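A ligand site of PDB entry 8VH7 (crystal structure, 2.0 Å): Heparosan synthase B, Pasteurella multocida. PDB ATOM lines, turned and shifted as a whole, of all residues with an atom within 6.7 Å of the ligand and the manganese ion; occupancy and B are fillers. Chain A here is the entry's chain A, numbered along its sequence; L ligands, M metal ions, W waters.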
ATOM      1  N   ILE A 305      -0.662   2.554   5.743  1.00  0.00           N
ATOM      2  CA  ILE A 305      -0.712   3.560   4.696  1.00  0.00           C
ATOM      3  C   ILE A 305       0.351   4.616   4.943  1.00  0.00           C
ATOM      4  O   ILE A 305       0.674   4.952   6.094  1.00  0.00           O
ATOM      5  CB  ILE A 305      -2.133   4.183   4.589  1.00  0.00           C
ATOM      6  CG1 ILE A 305      -2.229   5.077   3.343  1.00  0.00           C
ATOM      7  CG2 ILE A 305      -2.521   4.922   5.884  1.00  0.00           C
ATOM      8  CD1 ILE A 305      -3.640   5.485   2.984  1.00  0.00           C
ATOM      9  N   CYS A 306       0.902   5.132   3.846  1.00  0.00           N
ATOM     10  CA  CYS A 306       1.801   6.266   3.821  1.00  0.00           C
ATOM     11  C   CYS A 306       1.113   7.421   3.120  1.00  0.00           C
ATOM     12  O   CYS A 306       0.305   7.216   2.199  1.00  0.00           O
ATOM     13  CB  CYS A 306       3.108   5.940   3.082  1.00  0.00           C
ATOM     14  SG  CYS A 306       3.977   4.535   3.738  1.00  0.00           S
ATOM     15  N   SER A 307       1.447   8.643   3.534  1.00  0.00           N
ATOM     16  CA  SER A 307       0.749   9.798   2.994  1.00  0.00           C
ATOM     17  C   SER A 307       1.658  11.013   2.961  1.00  0.00           C
ATOM     18  O   SER A 307       2.474  11.213   3.862  1.00  0.00           O
ATOM     19  CB  SER A 307      -0.522  10.106   3.794  1.00  0.00           C
ATOM     20  OG  SER A 307      -1.252  11.182   3.212  1.00  0.00           O
ATOM     21  N   ILE A 308       1.504  11.811   1.908  1.00  0.00           N
ATOM     22  CA  ILE A 308       2.204  13.072   1.739  1.00  0.00           C
ATOM     23  C   ILE A 308       1.177  14.201   1.839  1.00  0.00           C
ATOM     24  O   ILE A 308       0.002  13.980   1.519  1.00  0.00           O
ATOM     25  CB  ILE A 308       2.996  13.112   0.425  1.00  0.00           C
ATOM     26  CG1 ILE A 308       2.088  12.901  -0.803  1.00  0.00           C
ATOM     27  CG2 ILE A 308       4.083  12.050   0.457  1.00  0.00           C
ATOM     28  CD1 ILE A 308       2.820  12.952  -2.136  1.00  0.00           C
ATOM     29  N   ARG A 311      -1.797  15.174  -0.536  1.00  0.00           N
ATOM     30  CA  ARG A 311      -2.921  14.262  -0.673  1.00  0.00           C
ATOM     31  C   ARG A 311      -3.790  14.192   0.587  1.00  0.00           C
ATOM     32  O   ARG A 311      -4.493  13.195   0.791  1.00  0.00           O
ATOM     33  CB  ARG A 311      -2.407  12.874  -1.038  1.00  0.00           C
ATOM     34  CG  ARG A 311      -1.679  12.805  -2.390  1.00  0.00           C
ATOM     35  CD  ARG A 311      -0.991  11.474  -2.597  1.00  0.00           C
ATOM     36  NE  ARG A 311      -0.296  11.404  -3.877  1.00  0.00           N
ATOM     37  CZ  ARG A 311       0.254  10.300  -4.381  1.00  0.00           C
ATOM     38  NH1 ARG A 311       0.212   9.145  -3.738  1.00  0.00           N
ATOM     39  NH2 ARG A 311       0.844  10.368  -5.569  1.00  0.00           N
ATOM     40  N   TYR A 332       1.937   6.293   8.357  1.00  0.00           N
ATOM     41  CA  TYR A 332       3.236   6.943   8.210  1.00  0.00           C
ATOM     42  C   TYR A 332       3.007   8.283   7.501  1.00  0.00           C
ATOM     43  O   TYR A 332       2.806   8.337   6.288  1.00  0.00           O
ATOM     44  CB  TYR A 332       4.165   6.015   7.432  1.00  0.00           C
ATOM     45  CG  TYR A 332       5.558   6.550   7.261  1.00  0.00           C
ATOM     46  CD1 TYR A 332       6.486   6.461   8.295  1.00  0.00           C
ATOM     47  CD2 TYR A 332       5.950   7.129   6.074  1.00  0.00           C
ATOM     48  CE1 TYR A 332       7.768   6.933   8.135  1.00  0.00           C
ATOM     49  CE2 TYR A 332       7.235   7.609   5.903  1.00  0.00           C
ATOM     50  CZ  TYR A 332       8.141   7.518   6.938  1.00  0.00           C
ATOM     51  OH  TYR A 332       9.413   7.992   6.768  1.00  0.00           O
ATOM     52  N   LEU A 333       3.031   9.365   8.283  1.00  0.00           N
ATOM     53  CA  LEU A 333       2.806  10.712   7.745  1.00  0.00           C
ATOM     54  C   LEU A 333       4.161  11.318   7.398  1.00  0.00           C
ATOM     55  O   LEU A 333       4.951  11.645   8.278  1.00  0.00           O
ATOM     56  CB  LEU A 333       2.059  11.582   8.751  1.00  0.00           C
ATOM     57  CG  LEU A 333       0.672  11.138   9.175  1.00  0.00           C
ATOM     58  CD1 LEU A 333       0.164  12.094  10.243  1.00  0.00           C
ATOM     59  CD2 LEU A 333      -0.318  11.074   7.997  1.00  0.00           C
ATOM     60  N   ASP A 334       4.398  11.503   6.104  1.00  0.00           N
ATOM     61  CA  ASP A 334       5.697  11.917   5.587  1.00  0.00           C
ATOM     62  C   ASP A 334       5.608  13.388   5.181  1.00  0.00           C
ATOM     63  O   ASP A 334       5.146  13.707   4.076  1.00  0.00           O
ATOM     64  CB  ASP A 334       6.123  11.027   4.425  1.00  0.00           C
ATOM     65  CG  ASP A 334       7.534  11.315   3.945  1.00  0.00           C
ATOM     66  OD1 ASP A 334       8.119  12.356   4.305  1.00  0.00           O
ATOM     67  OD2 ASP A 334       8.091  10.475   3.215  1.00  0.00           O
ATOM     68  N   SER A 361      13.249  10.128   5.839  1.00  0.00           N
ATOM     69  CA  SER A 361      12.081   9.494   5.235  1.00  0.00           C
ATOM     70  C   SER A 361      12.455   8.191   4.547  1.00  0.00           C
ATOM     71  O   SER A 361      13.469   8.103   3.848  1.00  0.00           O
ATOM     72  CB  SER A 361      11.449  10.441   4.219  1.00  0.00           C
ATOM     73  OG  SER A 361      10.214   9.934   3.737  1.00  0.00           O
ATOM     74  N   ILE A 362      11.640   7.155   4.790  1.00  0.00           N
ATOM     75  CA  ILE A 362      11.694   5.915   4.019  1.00  0.00           C
ATOM     76  C   ILE A 362      10.556   5.799   3.023  1.00  0.00           C
ATOM     77  O   ILE A 362      10.435   4.767   2.351  1.00  0.00           O
ATOM     78  CB  ILE A 362      11.749   4.677   4.947  1.00  0.00           C
ATOM     79  CG1 ILE A 362      10.524   4.582   5.873  1.00  0.00           C
ATOM     80  CG2 ILE A 362      13.035   4.683   5.765  1.00  0.00           C
ATOM     81  CD1 ILE A 362      10.448   3.260   6.644  1.00  0.00           C
ATOM     82  N   ARG A 363       9.715   6.832   2.923  1.00  0.00           N
ATOM     83  CA  ARG A 363       8.665   6.938   1.903  1.00  0.00           C
ATOM     84  C   ARG A 363       7.770   5.704   1.916  1.00  0.00           C
ATOM     85  O   ARG A 363       7.243   5.359   2.977  1.00  0.00           O
ATOM     86  CB  ARG A 363       9.318   7.199   0.533  1.00  0.00           C
ATOM     87  CG  ARG A 363      10.316   8.365   0.562  1.00  0.00           C
ATOM     88  CD  ARG A 363      10.650   8.879  -0.828  1.00  0.00           C
ATOM     89  NE  ARG A 363      11.482   7.949  -1.591  1.00  0.00           N
ATOM     90  CZ  ARG A 363      11.777   8.090  -2.874  1.00  0.00           C
ATOM     91  NH1 ARG A 363      11.285   9.090  -3.599  1.00  0.00           N
ATOM     92  NH2 ARG A 363      12.574   7.204  -3.459  1.00  0.00           N
ATOM     93  N   ASP A 364       7.596   5.009   0.783  1.00  0.00           N
ATOM     94  CA  ASP A 364       6.643   3.903   0.676  1.00  0.00           C
ATOM     95  C   ASP A 364       7.082   2.659   1.437  1.00  0.00           C
ATOM     96  O   ASP A 364       6.266   1.760   1.647  1.00  0.00           O
ATOM     97  CB  ASP A 364       6.396   3.546  -0.798  1.00  0.00           C
ATOM     98  CG  ASP A 364       7.690   3.242  -1.569  1.00  0.00           C
ATOM     99  OD1 ASP A 364       8.755   3.754  -1.161  1.00  0.00           O
ATOM    100  OD2 ASP A 364       7.628   2.528  -2.585  1.00  0.00           O
ATOM    101  N   ASN A 365       8.347   2.588   1.882  1.00  0.00           N
ATOM    102  CA  ASN A 365       8.716   1.494   2.782  1.00  0.00           C
ATOM    103  C   ASN A 365       7.992   1.571   4.123  1.00  0.00           C
ATOM    104  O   ASN A 365       8.020   0.594   4.867  1.00  0.00           O
ATOM    105  CB  ASN A 365      10.226   1.475   3.000  1.00  0.00           C
ATOM    106  CG  ASN A 365      11.001   1.034   1.771  1.00  0.00           C
ATOM    107  OD1 ASN A 365      10.448   0.437   0.856  1.00  0.00           O
ATOM    108  ND2 ASN A 365      12.297   1.321   1.759  1.00  0.00           N
ATOM    109  N   LYS A 367       4.946   1.364   4.596  1.00  0.00           N
ATOM    110  CA  LYS A 367       3.862   0.387   4.604  1.00  0.00           C
ATOM    111  C   LYS A 367       4.252  -0.898   5.311  1.00  0.00           C
ATOM    112  O   LYS A 367       3.359  -1.670   5.703  1.00  0.00           O
ATOM    113  CB  LYS A 367       3.429   0.075   3.174  1.00  0.00           C
ATOM    114  CG  LYS A 367       2.588   1.168   2.535  1.00  0.00           C
ATOM    115  CD  LYS A 367       2.255   0.866   1.060  1.00  0.00           C
ATOM    116  CE  LYS A 367       3.183   1.627   0.114  1.00  0.00           C
ATOM    117  NZ  LYS A 367       2.946   1.323  -1.335  1.00  0.00           N
ATOM    118  N   CYS A 386      -2.100   0.091   1.703  1.00  0.00           N
ATOM    119  CA  CYS A 386      -2.898   1.022   0.927  1.00  0.00           C
ATOM    120  C   CYS A 386      -2.055   2.240   0.585  1.00  0.00           C
ATOM    121  O   CYS A 386      -1.019   2.484   1.201  1.00  0.00           O
ATOM    122  CB  CYS A 386      -4.154   1.450   1.695  1.00  0.00           C
ATOM    123  SG  CYS A 386      -5.252   0.078   2.082  1.00  0.00           S
ATOM    124  N   ASP A 387      -2.498   2.984  -0.420  1.00  0.00           N
ATOM    125  CA  ASP A 387      -1.881   4.229  -0.835  1.00  0.00           C
ATOM    126  C   ASP A 387      -2.882   5.369  -0.737  1.00  0.00           C
ATOM    127  O   ASP A 387      -4.096   5.155  -0.836  1.00  0.00           O
ATOM    128  CB  ASP A 387      -1.334   4.168  -2.270  1.00  0.00           C
ATOM    129  CG  ASP A 387      -0.063   3.330  -2.398  1.00  0.00           C
ATOM    130  OD1 ASP A 387       0.490   2.890  -1.375  1.00  0.00           O
ATOM    131  OD2 ASP A 387       0.366   3.130  -3.554  1.00  0.00           O
ATOM    132  N   ASP A 388      -2.355   6.593  -0.593  1.00  0.00           N
ATOM    133  CA  ASP A 388      -3.180   7.769  -0.316  1.00  0.00           C
ATOM    134  C   ASP A 388      -3.670   8.482  -1.578  1.00  0.00           C
ATOM    135  O   ASP A 388      -4.020   9.664  -1.512  1.00  0.00           O
ATOM    136  CB  ASP A 388      -2.413   8.744   0.575  1.00  0.00           C
ATOM    137  CG  ASP A 388      -1.201   9.348  -0.097  1.00  0.00           C
ATOM    138  OD1 ASP A 388      -0.652   8.737  -1.029  1.00  0.00           O
ATOM    139  OD2 ASP A 388      -0.807  10.450   0.326  1.00  0.00           O
ATOM    140  N   ASP A 389      -3.727   7.784  -2.716  1.00  0.00           N
ATOM    141  CA  ASP A 389      -4.260   8.332  -3.961  1.00  0.00           C
ATOM    142  C   ASP A 389      -5.252   7.354  -4.611  1.00  0.00           C
ATOM    143  O   ASP A 389      -5.409   7.357  -5.830  1.00  0.00           O
ATOM    144  CB  ASP A 389      -3.140   8.680  -4.937  1.00  0.00           C
ATOM    145  CG  ASP A 389      -2.307   7.474  -5.343  1.00  0.00           C
ATOM    146  OD1 ASP A 389      -2.511   6.375  -4.778  1.00  0.00           O
ATOM    147  OD2 ASP A 389      -1.443   7.608  -6.237  1.00  0.00           O
ATOM    148  N   ILE A 390      -5.908   6.523  -3.811  1.00  0.00           N
ATOM    149  CA  ILE A 390      -6.863   5.528  -4.289  1.00  0.00           C
ATOM    150  C   ILE A 390      -8.174   5.707  -3.526  1.00  0.00           C
ATOM    151  O   ILE A 390      -8.177   6.034  -2.340  1.00  0.00           O
ATOM    152  CB  ILE A 390      -6.313   4.086  -4.138  1.00  0.00           C
ATOM    153  CG1 ILE A 390      -5.099   3.907  -5.048  1.00  0.00           C
ATOM    154  CG2 ILE A 390      -7.395   3.009  -4.443  1.00  0.00           C
ATOM    155  CD1 ILE A 390      -4.326   2.619  -4.851  1.00  0.00           C
ATOM    156  N   PHE A 437      -5.322  -1.434 -11.435  1.00  0.00           N
ATOM    157  CA  PHE A 437      -6.270  -1.809 -10.384  1.00  0.00           C
ATOM    158  C   PHE A 437      -7.700  -1.342 -10.667  1.00  0.00           C
ATOM    159  O   PHE A 437      -8.651  -1.936 -10.148  1.00  0.00           O
ATOM    160  CB  PHE A 437      -5.784  -1.254  -9.019  1.00  0.00           C
ATOM    161  CG  PHE A 437      -5.729   0.246  -8.931  1.00  0.00           C
ATOM    162  CD1 PHE A 437      -6.872   0.996  -8.660  1.00  0.00           C
ATOM    163  CD2 PHE A 437      -4.531   0.916  -9.066  1.00  0.00           C
ATOM    164  CE1 PHE A 437      -6.824   2.371  -8.560  1.00  0.00           C
ATOM    165  CE2 PHE A 437      -4.466   2.305  -8.967  1.00  0.00           C
ATOM    166  CZ  PHE A 437      -5.620   3.026  -8.713  1.00  0.00           C
ATOM    167  N   GLY A 474      11.169   4.062  -2.390  1.00  0.00           N
ATOM    168  CA  GLY A 474      10.569   4.307  -3.674  1.00  0.00           C
ATOM    169  C   GLY A 474      10.361   3.084  -4.535  1.00  0.00           C
ATOM    170  O   GLY A 474       9.951   3.235  -5.698  1.00  0.00           O
ATOM    171  N   ASP A 477       7.128  -2.040  -4.046  1.00  0.00           N
ATOM    172  CA  ASP A 477       6.513  -3.123  -4.793  1.00  0.00           C
ATOM    173  C   ASP A 477       7.549  -4.169  -5.192  1.00  0.00           C
ATOM    174  O   ASP A 477       7.310  -5.378  -5.059  1.00  0.00           O
ATOM    175  CB  ASP A 477       5.816  -2.609  -6.047  1.00  0.00           C
ATOM    176  CG  ASP A 477       4.723  -1.596  -5.763  1.00  0.00           C
ATOM    177  OD1 ASP A 477       4.255  -1.521  -4.604  1.00  0.00           O
ATOM    178  OD2 ASP A 477       4.333  -0.878  -6.718  1.00  0.00           O
ATOM    179  N   ASN A 505      -5.416  10.945  -8.086  1.00  0.00           N
ATOM    180  CA  ASN A 505      -4.110  11.584  -8.012  1.00  0.00           C
ATOM    181  C   ASN A 505      -4.234  13.094  -7.896  1.00  0.00           C
ATOM    182  O   ASN A 505      -3.353  13.739  -7.321  1.00  0.00           O
ATOM    183  CB  ASN A 505      -3.265  11.214  -9.230  1.00  0.00           C
ATOM    184  N   SER A 508      -1.411  15.565  -7.928  1.00  0.00           N
ATOM    185  CA  SER A 508      -0.359  15.435  -6.926  1.00  0.00           C
ATOM    186  C   SER A 508       1.032  15.210  -7.528  1.00  0.00           C
ATOM    187  O   SER A 508       1.215  15.284  -8.739  1.00  0.00           O
ATOM    188  CB  SER A 508      -0.682  14.274  -5.969  1.00  0.00           C
ATOM    189  OG  SER A 508       0.453  13.922  -5.211  1.00  0.00           O
HETATM  190  N1  LIG L   1       4.957   8.344  -0.632  1.00  0.00           N
HETATM  191  C1  LIG L   1       5.588   8.806   0.514  1.00  0.00           C
HETATM  192  N2  LIG L   1       6.655   9.635   0.280  1.00  0.00           N
HETATM  193  C2  LIG L   1       7.151  10.040  -0.936  1.00  0.00           C
HETATM  194  C3  LIG L   1       6.458   9.528  -2.074  1.00  0.00           C
HETATM  195  C4  LIG L   1       5.419   8.717  -1.873  1.00  0.00           C
HETATM  196  O1  LIG L   1       5.244   8.516   1.652  1.00  0.00           O
HETATM  197  O2  LIG L   1       8.123  10.788  -0.967  1.00  0.00           O
HETATM  198  C5  LIG L   1       3.793   7.435  -0.496  1.00  0.00           C
HETATM  199  C6  LIG L   1       2.509   7.977  -1.145  1.00  0.00           C
HETATM  200  O3  LIG L   1       1.789   8.753  -0.201  1.00  0.00           O
HETATM  201  C7  LIG L   1       1.797   6.667  -1.454  1.00  0.00           C
HETATM  202  C8  LIG L   1       2.924   5.689  -1.793  1.00  0.00           C
HETATM  203  O4  LIG L   1       4.107   6.223  -1.150  1.00  0.00           O
HETATM  204  O5  LIG L   1       0.984   6.253  -0.374  1.00  0.00           O
HETATM  205  C9  LIG L   1       3.208   5.533  -3.258  1.00  0.00           C
HETATM  206  O6  LIG L   1       3.341   6.832  -3.838  1.00  0.00           O
HETATM  207  P1  LIG L   1       2.838   7.136  -5.323  1.00  0.00           P
HETATM  208  O7  LIG L   1       3.438   8.418  -5.760  1.00  0.00           O
HETATM  209  O8  LIG L   1       1.357   7.059  -5.332  1.00  0.00           O
HETATM  210  O9  LIG L   1       3.501   5.912  -6.121  1.00  0.00           O
HETATM  211  P2  LIG L   1       3.063   5.318  -7.575  1.00  0.00           P
HETATM  212  O10 LIG L   1       1.608   4.977  -7.440  1.00  0.00           O
HETATM  213  O11 LIG L   1       3.890   4.092  -7.808  1.00  0.00           O
HETATM  214  O12 LIG L   1       3.347   6.462  -8.529  1.00  0.00           O
HETATM  215 MN    MN M   1       0.070   6.164  -6.780  1.00  0.00          MN
HETATM  216  O   HOH W   1       1.210   3.989   1.356  1.00  0.00           O
HETATM  217  O   HOH W   2       9.146  11.752  -2.962  1.00  0.00           O
HETATM  218  O   HOH W   3      -1.534   5.397  -8.579  1.00  0.00           O
HETATM  219  O   HOH W   4      -0.647   4.680  -5.454  1.00  0.00           O
HETATM  220  O   HOH W   5       0.823   7.744  -8.368  1.00  0.00           O
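Water W4 bridges the side-chain carboxylate of Asp 389 and the side-chain carboxylate of Asp 387.
Water W2 lies within hydrogen-bond range of an oxygen (O2) of the ligand (2.4 Å) and the guanidinium group (NH1) of Arg 363 (3.5 Å).
Water W1 lies within hydrogen-bond range of the backbone carbonyl oxygen (O) of Cys 386 (2.7 Å), the backbone NH (N) of Cys 306 (2.8 Å), an oxygen (O5) of the ligand (2.9 Å) and the side-chain carboxylate (OD1) of Asp 387 (3.0 Å).
Within 4 Å of the manganese ion: Asp 389.
The nearest printed residue that does not touch the manganese ion is Arg 311 (4.3 Å).
The side-chain carboxylate (OD2) of Asp 389 sits close to the guanidinium group (NH1) of Arg 311 (3.4 Å).
NH1 of Arg 311 is in salt-bridge range of OD1 of Asp 388 (2.9 Å).
O of Arg 363 lies within hydrogen-bond range of SG of Cys 306, 3.5 Å away.
The guanidinium group (NE) of Arg 311 lies within hydrogen-bond range of the side-chain hydroxyl (OG) of Ser 508, 2.9 Å away.
The backbone NH (N) of Arg 363 sits at hydrogen-bond distance from the side-chain hydroxyl (OG) of Ser 361.
N of Asp 334 is in hydrogen-bond range of O of Ser 307 (3.0 Å).
The side-chain carboxylate (OD1) of Asp 334 lies close to the side-chain hydroxyl (OG) of Ser 361 (3.3 Å).
N of Ser 307 sits at hydrogen-bond distance from O of Tyr 332 (3.1 Å).
O5 of the ligand is in hydrogen-bond range of N of Asp 388, at 3.4 Å.
O3 of the ligand is in hydrogen-bond range of OD1 of Asp 388, at 2.6 Å.
O of Cys 306 lies within hydrogen-bond range of O5 of the ligand (2.8 Å).
NH2 of Arg 311 is in salt-bridge range of O7 of the ligand (3.3 Å).
The side-chain carboxylate (OD2) of Asp 334 sits at hydrogen-bond distance from a nitrogen (N2) of the ligand, 3.4 Å away.
The manganese ion is bound by an oxygen (O10) of the ligand (2.1 Å), water W4 (2.1 Å), an oxygen (O8) of the ligand (2.1 Å), the side-chain carboxylate (OD2) of Asp 389 (2.2 Å), water W5 (2.4 Å) and water W3 (2.5 Å).
The manganese ion has six donor atoms within binding distance.
CA of Ser 307 touches O3 of the ligand, 3.5 Å away.
Ile 308 touches the ligand (CG2 to N2, 3.5 Å).
CD of Arg 363 touches O2 of the ligand, 3.2 Å away.
Asp 364 touches the ligand (CB to O4, 3.5 Å).
Asp 387 touches the ligand.
Hydrophobic or aromatic side chains that line the ligand: Ile 308.
Within 4 Å of the ligand: Cys 306, Ser 307, Ile 308, Arg 311, Asp 334, Arg 363, Asp 364, Asp 387, Asp 388 and Asp 389.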
